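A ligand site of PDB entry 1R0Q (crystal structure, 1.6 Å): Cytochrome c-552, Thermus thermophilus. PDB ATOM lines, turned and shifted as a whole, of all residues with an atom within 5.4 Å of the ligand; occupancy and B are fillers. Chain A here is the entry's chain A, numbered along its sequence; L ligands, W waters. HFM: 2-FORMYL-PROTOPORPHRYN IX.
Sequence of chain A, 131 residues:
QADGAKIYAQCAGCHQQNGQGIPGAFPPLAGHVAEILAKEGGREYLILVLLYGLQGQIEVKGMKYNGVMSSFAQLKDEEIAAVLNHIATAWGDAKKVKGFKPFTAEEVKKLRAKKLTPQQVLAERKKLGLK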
ATOM      1  N   ILE A   7       3.103  14.709  17.007  1.00  0.00           N
ATOM      2  CA  ILE A   7       3.737  14.359  15.732  1.00  0.00           C
ATOM      3  C   ILE A   7       4.786  13.264  15.944  1.00  0.00           C
ATOM      4  O   ILE A   7       4.867  12.241  15.256  1.00  0.00           O
ATOM      5  CB  ILE A   7       4.408  15.572  15.072  1.00  0.00           C
ATOM      6  CG1 ILE A   7       3.416  16.682  14.685  1.00  0.00           C
ATOM      7  CG2 ILE A   7       5.230  15.161  13.860  1.00  0.00           C
ATOM      8  CD1 ILE A   7       4.049  18.052  14.671  1.00  0.00           C
ATOM      9  N   TYR A   8       5.640  13.463  16.942  1.00  0.00           N
ATOM     10  CA  TYR A   8       6.654  12.445  17.185  1.00  0.00           C
ATOM     11  C   TYR A   8       6.029  11.097  17.529  1.00  0.00           C
ATOM     12  O   TYR A   8       6.536  10.048  17.115  1.00  0.00           O
ATOM     13  CB  TYR A   8       7.585  12.908  18.309  1.00  0.00           C
ATOM     14  CG  TYR A   8       8.627  11.855  18.606  1.00  0.00           C
ATOM     15  CD1 TYR A   8       8.560  11.047  19.741  1.00  0.00           C
ATOM     16  CD2 TYR A   8       9.690  11.676  17.721  1.00  0.00           C
ATOM     17  CE1 TYR A   8       9.536  10.082  19.989  1.00  0.00           C
ATOM     18  CE2 TYR A   8      10.657  10.713  17.978  1.00  0.00           C
ATOM     19  CZ  TYR A   8      10.590   9.922  19.091  1.00  0.00           C
ATOM     20  OH  TYR A   8      11.576   8.971  19.296  1.00  0.00           O
ATOM     21  N   CYS A  11       5.464   9.126  14.824  1.00  0.00           N
ATOM     22  CA  CYS A  11       6.643   8.618  14.089  1.00  0.00           C
ATOM     23  C   CYS A  11       7.633   7.997  15.048  1.00  0.00           C
ATOM     24  O   CYS A  11       8.831   8.025  14.787  1.00  0.00           O
ATOM     25  N   GLY A  13       8.068   4.788  16.075  1.00  0.00           N
ATOM     26  CA  GLY A  13       8.241   3.347  16.014  1.00  0.00           C
ATOM     27  C   GLY A  13       9.690   2.921  16.006  1.00  0.00           C
ATOM     28  O   GLY A  13      10.037   1.762  16.317  1.00  0.00           O
ATOM     29  N   CYS A  14      10.564   3.870  15.647  1.00  0.00           N
ATOM     30  CA  CYS A  14      11.976   3.524  15.549  1.00  0.00           C
ATOM     31  C   CYS A  14      12.790   4.031  16.721  1.00  0.00           C
ATOM     32  O   CYS A  14      13.425   3.243  17.430  1.00  0.00           O
ATOM     33  CB  CYS A  14      12.536   4.080  14.220  1.00  0.00           C
ATOM     34  SG  CYS A  14      11.749   3.236  12.789  1.00  0.00           S
ATOM     35  N   HIS A  15      12.784   5.350  16.924  1.00  0.00           N
ATOM     36  CA  HIS A  15      13.579   5.899  18.030  1.00  0.00           C
ATOM     37  C   HIS A  15      12.896   5.676  19.390  1.00  0.00           C
ATOM     38  O   HIS A  15      13.589   5.844  20.398  1.00  0.00           O
ATOM     39  CB  HIS A  15      13.872   7.380  17.810  1.00  0.00           C
ATOM     40  CG  HIS A  15      14.596   7.607  16.499  1.00  0.00           C
ATOM     41  ND1 HIS A  15      15.931   7.337  16.334  1.00  0.00           N
ATOM     42  CD2 HIS A  15      14.124   8.072  15.313  1.00  0.00           C
ATOM     43  CE1 HIS A  15      16.269   7.642  15.084  1.00  0.00           C
ATOM     44  NE2 HIS A  15      15.207   8.087  14.452  1.00  0.00           N
ATOM     45  N   ALA A  25      20.131  -0.749  15.863  1.00  0.00           N
ATOM     46  CA  ALA A  25      19.158  -0.516  14.802  1.00  0.00           C
ATOM     47  C   ALA A  25      18.789   0.947  14.574  1.00  0.00           C
ATOM     48  O   ALA A  25      18.843   1.486  13.464  1.00  0.00           O
ATOM     49  CB  ALA A  25      17.893  -1.292  15.181  1.00  0.00           C
ATOM     50  N   PHE A  26      18.346   1.585  15.654  1.00  0.00           N
ATOM     51  CA  PHE A  26      17.785   2.935  15.577  1.00  0.00           C
ATOM     52  C   PHE A  26      18.524   3.790  16.605  1.00  0.00           C
ATOM     53  O   PHE A  26      18.455   3.497  17.815  1.00  0.00           O
ATOM     54  CB  PHE A  26      16.285   2.879  15.810  1.00  0.00           C
ATOM     55  CG  PHE A  26      15.542   1.926  14.875  1.00  0.00           C
ATOM     56  CD1 PHE A  26      15.677   2.032  13.496  1.00  0.00           C
ATOM     57  CD2 PHE A  26      14.730   0.933  15.390  1.00  0.00           C
ATOM     58  CE1 PHE A  26      15.022   1.175  12.637  1.00  0.00           C
ATOM     59  CE2 PHE A  26      14.085   0.075  14.531  1.00  0.00           C
ATOM     60  CZ  PHE A  26      14.209   0.172  13.153  1.00  0.00           C
ATOM     61  N   PRO A  27      19.271   4.813  16.219  1.00  0.00           N
ATOM     62  CA  PRO A  27      20.090   5.481  17.239  1.00  0.00           C
ATOM     63  C   PRO A  27      19.211   6.248  18.215  1.00  0.00           C
ATOM     64  O   PRO A  27      18.074   6.654  17.953  1.00  0.00           O
ATOM     65  CB  PRO A  27      20.964   6.443  16.434  1.00  0.00           C
ATOM     66  CG  PRO A  27      20.169   6.705  15.202  1.00  0.00           C
ATOM     67  CD  PRO A  27      19.472   5.406  14.886  1.00  0.00           C
ATOM     68  N   LEU A  29      17.858   9.275  20.466  1.00  0.00           N
ATOM     69  CA  LEU A  29      17.733  10.734  20.382  1.00  0.00           C
ATOM     70  C   LEU A  29      17.975  11.335  21.750  1.00  0.00           C
ATOM     71  O   LEU A  29      18.740  12.272  21.950  1.00  0.00           O
ATOM     72  CB  LEU A  29      16.356  11.083  19.822  1.00  0.00           C
ATOM     73  CG  LEU A  29      16.057  10.560  18.406  1.00  0.00           C
ATOM     74  CD1 LEU A  29      14.654  10.918  17.987  1.00  0.00           C
ATOM     75  CD2 LEU A  29      17.086  11.108  17.427  1.00  0.00           C
ATOM     76  N   HIS A  32      21.376  12.466  22.897  1.00  0.00           N
ATOM     77  CA  HIS A  32      22.247  12.572  21.718  1.00  0.00           C
ATOM     78  C   HIS A  32      21.942  13.799  20.872  1.00  0.00           C
ATOM     79  O   HIS A  32      22.778  14.364  20.180  1.00  0.00           O
ATOM     80  CB  HIS A  32      22.101  11.282  20.910  1.00  0.00           C
ATOM     81  CG  HIS A  32      22.752  11.287  19.569  1.00  0.00           C
ATOM     82  ND1 HIS A  32      24.078  11.629  19.375  1.00  0.00           N
ATOM     83  CD2 HIS A  32      22.259  11.009  18.338  1.00  0.00           C
ATOM     84  CE1 HIS A  32      24.387  11.568  18.093  1.00  0.00           C
ATOM     85  NE2 HIS A  32      23.300  11.183  17.438  1.00  0.00           N
ATOM     86  N   ILE A  36      24.618  16.735  18.933  1.00  0.00           N
ATOM     87  CA  ILE A  36      24.539  17.320  17.588  1.00  0.00           C
ATOM     88  C   ILE A  36      24.390  18.827  17.701  1.00  0.00           C
ATOM     89  O   ILE A  36      25.025  19.579  16.980  1.00  0.00           O
ATOM     90  CB  ILE A  36      23.368  16.723  16.822  1.00  0.00           C
ATOM     91  CG1 ILE A  36      23.592  15.233  16.473  1.00  0.00           C
ATOM     92  CG2 ILE A  36      23.029  17.482  15.543  1.00  0.00           C
ATOM     93  CD1 ILE A  36      22.323  14.538  16.005  1.00  0.00           C
ATOM     94  N   TYR A  45      21.528  20.567  10.529  1.00  0.00           N
ATOM     95  CA  TYR A  45      21.686  19.138  10.234  1.00  0.00           C
ATOM     96  C   TYR A  45      20.425  18.401  10.679  1.00  0.00           C
ATOM     97  O   TYR A  45      19.874  17.572   9.924  1.00  0.00           O
ATOM     98  CB  TYR A  45      22.973  18.572  10.875  1.00  0.00           C
ATOM     99  CG  TYR A  45      22.931  17.058  10.789  1.00  0.00           C
ATOM    100  CD1 TYR A  45      23.151  16.433   9.563  1.00  0.00           C
ATOM    101  CD2 TYR A  45      22.646  16.300  11.914  1.00  0.00           C
ATOM    102  CE1 TYR A  45      23.105  15.038   9.461  1.00  0.00           C
ATOM    103  CE2 TYR A  45      22.600  14.916  11.812  1.00  0.00           C
ATOM    104  CZ  TYR A  45      22.831  14.302  10.603  1.00  0.00           C
ATOM    105  OH  TYR A  45      22.758  12.936  10.550  1.00  0.00           O
ATOM    106  N   LEU A  46      19.938  18.713  11.884  1.00  0.00           N
ATOM    107  CA  LEU A  46      18.721  18.050  12.368  1.00  0.00           C
ATOM    108  C   LEU A  46      17.545  18.343  11.456  1.00  0.00           C
ATOM    109  O   LEU A  46      16.712  17.468  11.241  1.00  0.00           O
ATOM    110  CB  LEU A  46      18.385  18.474  13.785  1.00  0.00           C
ATOM    111  CG  LEU A  46      19.396  18.017  14.854  1.00  0.00           C
ATOM    112  CD1 LEU A  46      19.114  18.757  16.159  1.00  0.00           C
ATOM    113  CD2 LEU A  46      19.363  16.525  15.088  1.00  0.00           C
ATOM    114  N   VAL A  49      17.948  16.131   8.280  1.00  0.00           N
ATOM    115  CA  VAL A  49      17.556  14.718   8.444  1.00  0.00           C
ATOM    116  C   VAL A  49      16.062  14.544   8.318  1.00  0.00           C
ATOM    117  O   VAL A  49      15.539  13.651   7.622  1.00  0.00           O
ATOM    118  CB  VAL A  49      18.019  14.177   9.812  1.00  0.00           C
ATOM    119  CG1 VAL A  49      17.422  12.798  10.088  1.00  0.00           C
ATOM    120  CG2 VAL A  49      19.541  14.122   9.895  1.00  0.00           C
ATOM    121  N   LEU A  50      15.301  15.407   8.996  1.00  0.00           N
ATOM    122  CA  LEU A  50      13.840  15.299   8.850  1.00  0.00           C
ATOM    123  C   LEU A  50      13.334  15.596   7.445  1.00  0.00           C
ATOM    124  O   LEU A  50      12.416  14.938   6.931  1.00  0.00           O
ATOM    125  CB  LEU A  50      13.151  16.243   9.858  1.00  0.00           C
ATOM    126  CG  LEU A  50      12.866  15.576  11.214  1.00  0.00           C
ATOM    127  CD1 LEU A  50      11.784  14.509  11.060  1.00  0.00           C
ATOM    128  CD2 LEU A  50      14.140  14.993  11.796  1.00  0.00           C
ATOM    129  N   LEU A  54      18.392  10.046   5.775  1.00  0.00           N
ATOM    130  CA  LEU A  54      19.769   9.791   6.121  1.00  0.00           C
ATOM    131  C   LEU A  54      20.115   8.358   5.720  1.00  0.00           C
ATOM    132  O   LEU A  54      19.247   7.482   5.718  1.00  0.00           O
ATOM    133  CB  LEU A  54      20.041   9.953   7.625  1.00  0.00           C
ATOM    134  CG  LEU A  54      21.478   9.834   8.113  1.00  0.00           C
ATOM    135  CD1 LEU A  54      22.387  10.848   7.411  1.00  0.00           C
ATOM    136  CD2 LEU A  54      21.561  10.017   9.620  1.00  0.00           C
ATOM    137  N   GLN A  55      21.368   8.141   5.389  1.00  0.00           N
ATOM    138  CA  GLN A  55      21.873   6.804   5.164  1.00  0.00           C
ATOM    139  C   GLN A  55      23.364   6.823   5.491  1.00  0.00           C
ATOM    140  O   GLN A  55      23.945   7.901   5.617  1.00  0.00           O
ATOM    141  CB  GLN A  55      21.597   6.358   3.726  1.00  0.00           C
ATOM    142  CG  GLN A  55      22.417   7.141   2.694  1.00  0.00           C
ATOM    143  CD  GLN A  55      21.956   6.789   1.290  1.00  0.00           C
ATOM    144  OE1 GLN A  55      20.776   6.535   1.054  1.00  0.00           O
ATOM    145  NE2 GLN A  55      22.897   6.792   0.354  1.00  0.00           N
ATOM    146  N   GLY A  56      23.915   5.621   5.620  1.00  0.00           N
ATOM    147  CA  GLY A  56      25.340   5.410   5.787  1.00  0.00           C
ATOM    148  C   GLY A  56      25.761   5.027   7.186  1.00  0.00           C
ATOM    149  O   GLY A  56      24.987   5.141   8.153  1.00  0.00           O
ATOM    150  N   GLN A  57      27.013   4.578   7.319  1.00  0.00           N
ATOM    151  CA  GLN A  57      27.534   4.228   8.630  1.00  0.00           C
ATOM    152  C   GLN A  57      27.799   5.483   9.449  1.00  0.00           C
ATOM    153  O   GLN A  57      28.467   6.393   8.939  1.00  0.00           O
ATOM    154  CB  GLN A  57      28.831   3.421   8.515  1.00  0.00           C
ATOM    155  CG  GLN A  57      28.696   2.150   7.694  1.00  0.00           C
ATOM    156  CD  GLN A  57      30.050   1.619   7.239  1.00  0.00           C
ATOM    157  OE1 GLN A  57      30.825   1.155   8.083  1.00  0.00           O
ATOM    158  NE2 GLN A  57      30.305   1.689   5.942  1.00  0.00           N
ATOM    159  N   ILE A  58      27.284   5.456  10.668  1.00  0.00           N
ATOM    160  CA  ILE A  58      27.441   6.497  11.668  1.00  0.00           C
ATOM    161  C   ILE A  58      27.678   5.856  13.035  1.00  0.00           C
ATOM    162  O   ILE A  58      27.313   4.714  13.274  1.00  0.00           O
ATOM    163  CB  ILE A  58      26.221   7.416  11.817  1.00  0.00           C
ATOM    164  CG1 ILE A  58      24.970   6.664  12.314  1.00  0.00           C
ATOM    165  CG2 ILE A  58      25.932   8.172  10.538  1.00  0.00           C
ATOM    166  CD1 ILE A  58      23.814   7.576  12.664  1.00  0.00           C
ATOM    167  N   GLU A  59      28.280   6.645  13.895  1.00  0.00           N
ATOM    168  CA  GLU A  59      28.572   6.276  15.275  1.00  0.00           C
ATOM    169  C   GLU A  59      27.726   7.125  16.199  1.00  0.00           C
ATOM    170  O   GLU A  59      27.685   8.341  15.983  1.00  0.00           O
ATOM    171  CB  GLU A  59      30.062   6.489  15.547  1.00  0.00           C
ATOM    172  CG  GLU A  59      30.585   5.667  16.718  1.00  0.00           C
ATOM    173  CD  GLU A  59      32.106   5.791  16.778  1.00  0.00           C
ATOM    174  OE1 GLU A  59      32.767   5.217  15.885  1.00  0.00           O
ATOM    175  OE2 GLU A  59      32.583   6.475  17.715  1.00  0.00           O
ATOM    176  N   VAL A  60      27.083   6.486  17.168  1.00  0.00           N
ATOM    177  CA  VAL A  60      26.373   7.222  18.203  1.00  0.00           C
ATOM    178  C   VAL A  60      26.672   6.599  19.576  1.00  0.00           C
ATOM    179  O   VAL A  60      26.344   5.430  19.777  1.00  0.00           O
ATOM    180  CB  VAL A  60      24.848   7.258  17.971  1.00  0.00           C
ATOM    181  CG1 VAL A  60      24.150   7.979  19.128  1.00  0.00           C
ATOM    182  CG2 VAL A  60      24.501   7.900  16.647  1.00  0.00           C
ATOM    183  N   TYR A  65      25.862   2.302  13.658  1.00  0.00           N
ATOM    184  CA  TYR A  65      24.579   2.187  12.984  1.00  0.00           C
ATOM    185  C   TYR A  65      24.859   2.242  11.496  1.00  0.00           C
ATOM    186  O   TYR A  65      25.746   2.940  10.997  1.00  0.00           O
ATOM    187  CB  TYR A  65      23.552   3.260  13.380  1.00  0.00           C
ATOM    188  CG  TYR A  65      23.240   3.156  14.865  1.00  0.00           C
ATOM    189  CD1 TYR A  65      24.141   3.723  15.764  1.00  0.00           C
ATOM    190  CD2 TYR A  65      22.115   2.527  15.342  1.00  0.00           C
ATOM    191  CE1 TYR A  65      23.866   3.632  17.126  1.00  0.00           C
ATOM    192  CE2 TYR A  65      21.830   2.436  16.704  1.00  0.00           C
ATOM    193  CZ  TYR A  65      22.741   3.001  17.583  1.00  0.00           C
ATOM    194  OH  TYR A  65      22.517   2.935  18.929  1.00  0.00           O
ATOM    195  N   ASN A  66      24.100   1.448  10.773  1.00  0.00           N
ATOM    196  CA  ASN A  66      24.298   1.461   9.324  1.00  0.00           C
ATOM    197  C   ASN A  66      22.930   1.218   8.719  1.00  0.00           C
ATOM    198  O   ASN A  66      22.662   0.209   8.080  1.00  0.00           O
ATOM    199  CB  ASN A  66      25.326   0.424   8.893  1.00  0.00           C
ATOM    200  CG  ASN A  66      25.680   0.538   7.425  1.00  0.00           C
ATOM    201  OD1 ASN A  66      25.305   1.500   6.757  1.00  0.00           O
ATOM    202  ND2 ASN A  66      26.397  -0.461   6.928  1.00  0.00           N
ATOM    203  N   GLY A  67      22.076   2.203   8.980  1.00  0.00           N
ATOM    204  CA  GLY A  67      20.708   2.099   8.509  1.00  0.00           C
ATOM    205  C   GLY A  67      20.342   3.179   7.512  1.00  0.00           C
ATOM    206  O   GLY A  67      21.159   3.893   6.952  1.00  0.00           O
ATOM    207  N   VAL A  68      19.031   3.279   7.316  1.00  0.00           N
ATOM    208  CA  VAL A  68      18.403   4.270   6.470  1.00  0.00           C
ATOM    209  C   VAL A  68      17.222   4.926   7.176  1.00  0.00           C
ATOM    210  O   VAL A  68      16.401   4.275   7.829  1.00  0.00           O
ATOM    211  CB  VAL A  68      17.909   3.620   5.166  1.00  0.00           C
ATOM    212  CG1 VAL A  68      16.962   4.564   4.456  1.00  0.00           C
ATOM    213  CG2 VAL A  68      19.090   3.204   4.287  1.00  0.00           C
ATOM    214  N   MET A  69      17.098   6.246   7.029  1.00  0.00           N
ATOM    215  CA  MET A  69      15.890   6.877   7.538  1.00  0.00           C
ATOM    216  C   MET A  69      15.240   7.584   6.356  1.00  0.00           C
ATOM    217  O   MET A  69      15.945   8.189   5.541  1.00  0.00           O
ATOM    218  CB  MET A  69      16.218   7.856   8.663  1.00  0.00           C
ATOM    219  CG  MET A  69      14.988   8.664   9.119  1.00  0.00           C
ATOM    220  SD  MET A  69      15.448   9.776  10.465  1.00  0.00           S
ATOM    221  CE  MET A  69      14.160  11.022  10.392  1.00  0.00           C
ATOM    222  N   PHE A  72      10.963  12.942   5.779  1.00  0.00           N
ATOM    223  CA  PHE A  72       9.661  13.290   6.326  1.00  0.00           C
ATOM    224  C   PHE A  72       9.202  14.662   5.830  1.00  0.00           C
ATOM    225  O   PHE A  72       8.545  15.379   6.584  1.00  0.00           O
ATOM    226  CB  PHE A  72       9.692  13.226   7.857  1.00  0.00           C
ATOM    227  CG  PHE A  72       9.656  11.773   8.318  1.00  0.00           C
ATOM    228  CD1 PHE A  72      10.785  10.986   8.286  1.00  0.00           C
ATOM    229  CD2 PHE A  72       8.474  11.206   8.779  1.00  0.00           C
ATOM    230  CE1 PHE A  72      10.784   9.657   8.700  1.00  0.00           C
ATOM    231  CE2 PHE A  72       8.453   9.886   9.182  1.00  0.00           C
ATOM    232  CZ  PHE A  72       9.592   9.096   9.129  1.00  0.00           C
ATOM    233  N   VAL A  83       8.383  18.972  15.949  1.00  0.00           N
ATOM    234  CA  VAL A  83       8.934  17.665  16.354  1.00  0.00           C
ATOM    235  C   VAL A  83      10.392  17.770  16.792  1.00  0.00           C
ATOM    236  O   VAL A  83      10.867  17.098  17.703  1.00  0.00           O
ATOM    237  CB  VAL A  83       8.775  16.655  15.208  1.00  0.00           C
ATOM    238  CG1 VAL A  83       9.711  17.034  14.063  1.00  0.00           C
ATOM    239  CG2 VAL A  83       9.062  15.249  15.684  1.00  0.00           C
ATOM    240  N   LEU A  84      11.155  18.657  16.141  1.00  0.00           N
ATOM    241  CA  LEU A  84      12.530  18.898  16.574  1.00  0.00           C
ATOM    242  C   LEU A  84      12.566  19.587  17.927  1.00  0.00           C
ATOM    243  O   LEU A  84      13.459  19.282  18.717  1.00  0.00           O
ATOM    244  CB  LEU A  84      13.261  19.741  15.506  1.00  0.00           C
ATOM    245  CG  LEU A  84      13.533  18.974  14.215  1.00  0.00           C
ATOM    246  CD1 LEU A  84      14.159  19.896  13.170  1.00  0.00           C
ATOM    247  CD2 LEU A  84      14.426  17.752  14.478  1.00  0.00           C
ATOM    248  N   ILE A  87      12.040  16.559  20.361  1.00  0.00           N
ATOM    249  CA  ILE A  87      13.214  15.727  20.626  1.00  0.00           C
ATOM    250  C   ILE A  87      14.333  16.534  21.276  1.00  0.00           C
ATOM    251  O   ILE A  87      15.179  15.963  21.950  1.00  0.00           O
ATOM    252  CB  ILE A  87      13.750  15.040  19.357  1.00  0.00           C
ATOM    253  CG1 ILE A  87      14.407  15.972  18.320  1.00  0.00           C
ATOM    254  CG2 ILE A  87      12.640  14.204  18.720  1.00  0.00           C
ATOM    255  CD1 ILE A  87      15.092  15.178  17.212  1.00  0.00           C
ATOM    256  N   ARG A 125      26.476  15.591   7.940  1.00  0.00           N
ATOM    257  CA  ARG A 125      26.788  15.071   9.259  1.00  0.00           C
ATOM    258  C   ARG A 125      28.297  15.078   9.507  1.00  0.00           C
ATOM    259  O   ARG A 125      28.821  15.468  10.531  1.00  0.00           O
ATOM    260  CB  ARG A 125      26.265  13.631   9.400  1.00  0.00           C
ATOM    261  CG  ARG A 125      26.321  13.140  10.843  1.00  0.00           C
ATOM    262  CD  ARG A 125      25.797  11.704  10.933  1.00  0.00           C
ATOM    263  NE  ARG A 125      25.474  11.291  12.287  1.00  0.00           N
ATOM    264  CZ  ARG A 125      26.387  10.766  13.105  1.00  0.00           C
ATOM    265  NH1 ARG A 125      27.632  10.635  12.652  1.00  0.00           N
ATOM    266  NH2 ARG A 125      26.064  10.397  14.332  1.00  0.00           N
ATOM    267  N   LEU A 130      31.256  14.774  13.101  1.00  0.00           N
ATOM    268  CA  LEU A 130      30.713  13.544  13.680  1.00  0.00           C
ATOM    269  C   LEU A 130      31.171  12.317  12.886  1.00  0.00           C
ATOM    270  O   LEU A 130      31.237  12.375  11.656  1.00  0.00           O
ATOM    271  CB  LEU A 130      29.183  13.573  13.710  1.00  0.00           C
ATOM    272  CG  LEU A 130      28.514  14.533  14.695  1.00  0.00           C
ATOM    273  CD1 LEU A 130      26.994  14.440  14.560  1.00  0.00           C
ATOM    274  CD2 LEU A 130      28.952  14.264  16.129  1.00  0.00           C
HETATM  275 FE   HFM L   1      15.232   8.796  12.544  1.00  0.00          FE
HETATM  276  CHA HFM L   1      18.620   8.955  12.274  1.00  0.00           C
HETATM  277  CHB HFM L   1      15.184  11.817  14.012  1.00  0.00           C
HETATM  278  CHC HFM L   1      11.880   8.764  12.334  1.00  0.00           C
HETATM  279  CHD HFM L   1      15.361   5.582  11.564  1.00  0.00           C
HETATM  280  NA  HFM L   1      16.680  10.187  13.079  1.00  0.00           N
HETATM  281  NB  HFM L   1      13.769  10.066  13.129  1.00  0.00           N
HETATM  282  NC  HFM L   1      13.864   7.392  12.019  1.00  0.00           N
HETATM  283  ND  HFM L   1      16.724   7.513  11.950  1.00  0.00           N
HETATM  284  C1A HFM L   1      17.991  10.083  12.863  1.00  0.00           C
HETATM  285  C2A HFM L   1      18.644  11.218  13.373  1.00  0.00           C
HETATM  286  C3A HFM L   1      17.667  12.073  13.826  1.00  0.00           C
HETATM  287  C4A HFM L   1      16.443  11.366  13.590  1.00  0.00           C
HETATM  288  CMA HFM L   1      17.772  13.422  14.456  1.00  0.00           C
HETATM  289  CAA HFM L   1      20.138  11.554  13.115  1.00  0.00           C
HETATM  290  CBA HFM L   1      20.947  10.986  14.335  1.00  0.00           C
HETATM  291  CGA HFM L   1      22.453  11.043  13.951  1.00  0.00           C
HETATM  292  O1A HFM L   1      23.281  10.776  14.859  1.00  0.00           O
HETATM  293  O2A HFM L   1      22.827  11.553  12.895  1.00  0.00           O
HETATM  294  C1B HFM L   1      13.924  11.173  13.859  1.00  0.00           C
HETATM  295  C2B HFM L   1      12.690  11.807  14.066  1.00  0.00           C
HETATM  296  C3B HFM L   1      11.774  11.032  13.426  1.00  0.00           C
HETATM  297  C4B HFM L   1      12.435   9.909  12.966  1.00  0.00           C
HETATM  298  CMB HFM L   1      12.444  13.050  14.911  1.00  0.00           C
HETATM  299  CAB HFM L   1      10.311  11.202  13.477  1.00  0.00           C
HETATM  300  OAB HFM L   1       9.865  12.124  14.178  1.00  0.00           O
HETATM  301  C1C HFM L   1      12.530   7.520  12.102  1.00  0.00           C
HETATM  302  C2C HFM L   1      11.876   6.366  11.524  1.00  0.00           C
HETATM  303  C3C HFM L   1      12.848   5.374  11.643  1.00  0.00           C
HETATM  304  C4C HFM L   1      14.088   6.077  11.698  1.00  0.00           C
HETATM  305  CMC HFM L   1      10.309   6.268  11.562  1.00  0.00           C
HETATM  306  CAC HFM L   1      12.716   3.804  11.245  1.00  0.00           C
HETATM  307  CBC HFM L   1      11.870   3.499   9.977  1.00  0.00           C
HETATM  308  C1D HFM L   1      16.587   6.182  11.682  1.00  0.00           C
HETATM  309  C2D HFM L   1      17.813   5.596  11.450  1.00  0.00           C
HETATM  310  C3D HFM L   1      18.780   6.562  11.640  1.00  0.00           C
HETATM  311  C4D HFM L   1      18.028   7.763  11.890  1.00  0.00           C
HETATM  312  CMD HFM L   1      18.056   4.115  11.029  1.00  0.00           C
HETATM  313  CAD HFM L   1      20.259   6.461  11.277  1.00  0.00           C
HETATM  314  CBD HFM L   1      20.516   6.288   9.739  1.00  0.00           C
HETATM  315  CGD HFM L   1      21.891   5.728   9.377  1.00  0.00           C
HETATM  316  O1D HFM L   1      22.614   6.293   8.567  1.00  0.00           O
HETATM  317  O2D HFM L   1      22.298   4.817  10.058  1.00  0.00           O
HETATM  318  O   HOH W   1      15.472   2.260   9.599  1.00  0.00           O
HETATM  319  O   HOH W   2      12.335   6.215   8.221  1.00  0.00           O
HETATM  320  O   HOH W   3      11.095   6.722  15.192  1.00  0.00           O
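CAC of the ligand is bonded to SG of Cys 14 (1.9 Å).
FE of the ligand is bound by NE2 of His 15 (2.0 Å).
The side-chain sulfur (SD) of Met 69 is bound to an iron atom (FE) of the ligand, at 2.3 Å.
O1A of the ligand is in hydrogen-bond range of NE2 of His 32 (2.6 Å).
An oxygen (O1D) of the ligand is in hydrogen-bond range of the backbone NH (N) of Gly 56 (3.3 Å).
The backbone carbonyl oxygen (O) of Gly 56 lies close to an oxygen (O1D) of the ligand (2.7 Å).
OH of Tyr 45 lies within hydrogen-bond range of O2A of the ligand (2.7 Å).
NE of Arg 125 lies within salt-bridge range of O2A of the ligand (2.7 Å).
The backbone NH of Gly 67 is in hydrogen-bond range of an oxygen (O2D) of the ligand, 2.8 Å away.
A ring nitrogen (ND1) of His 15 is in hydrogen-bond range of the backbone carbonyl oxygen (O) of Pro 27, at 2.8 Å.
The backbone NH of Met 69 sits at hydrogen-bond distance from the backbone carbonyl oxygen of Leu 54 (2.8 Å).
The backbone carbonyl oxygen (O) of Glu 59 lies within hydrogen-bond range of the guanidinium group (NH2) of Arg 125.
The backbone carbonyl oxygen (O) of Leu 50 is in hydrogen-bond range of the backbone NH (N) of Phe 72 (2.7 Å).
N of Tyr 65 is in hydrogen-bond range of O of Ile 58 (2.8 Å).
CD2 of Tyr 8 touches OAB of the ligand (3.6 Å).
O of Cys 11 touches CAB of the ligand (3.7 Å).
Ala 25 touches the ligand.
Phe 26 touches the ligand (CE1 to CAC, 3.8 Å).
Pro 27 touches the ligand.
Leu 29 touches the ligand (CD2 to C3A, 3.8 Å).
Leu 46 touches the ligand.
Val 49 touches the ligand.
Leu 54 touches the ligand.
Gln 55 touches the ligand (C to O1D, 3.2 Å).
Ile 58 touches the ligand (CD1 to O1A, 3.9 Å).
Val 60 touches the ligand.
CB of Tyr 65 touches O2D of the ligand (3.9 Å).
Asn 66 touches the ligand (N to O2D, 3.9 Å).
Val 68 touches the ligand (O to CMD, 3.6 Å).
CZ of Phe 72 touches CMC of the ligand (3.8 Å).
Val 83 touches the ligand (CG2 to OAB, 3.6 Å).
Ile 87 touches the ligand.
Hydrophobic or aromatic side chains within 4 Å of the ligand: Tyr 8, His 15, Phe 26, Pro 27, Leu 29, His 32, Tyr 45, Leu 46, Val 49, Leu 54, Ile 58, Val 60, Tyr 65, Met 69, Phe 72, Val 83 and Ile 87.
Within 4 Å of the ligand: Tyr 8, Cys 11, Cys 14, His 15, Ala 25, Phe 26, Pro 27, Leu 29, His 32, Tyr 45, Leu 46, Val 49, Leu 54, Gln 55, Gly 56, Ile 58, Val 60, Tyr 65, Asn 66, Gly 67, Val 68, Met 69, Phe 72, Val 83, Ile 87 and Arg 125.
The nearest printed residue that does not touch the ligand is Leu 50 (4.01 Å).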
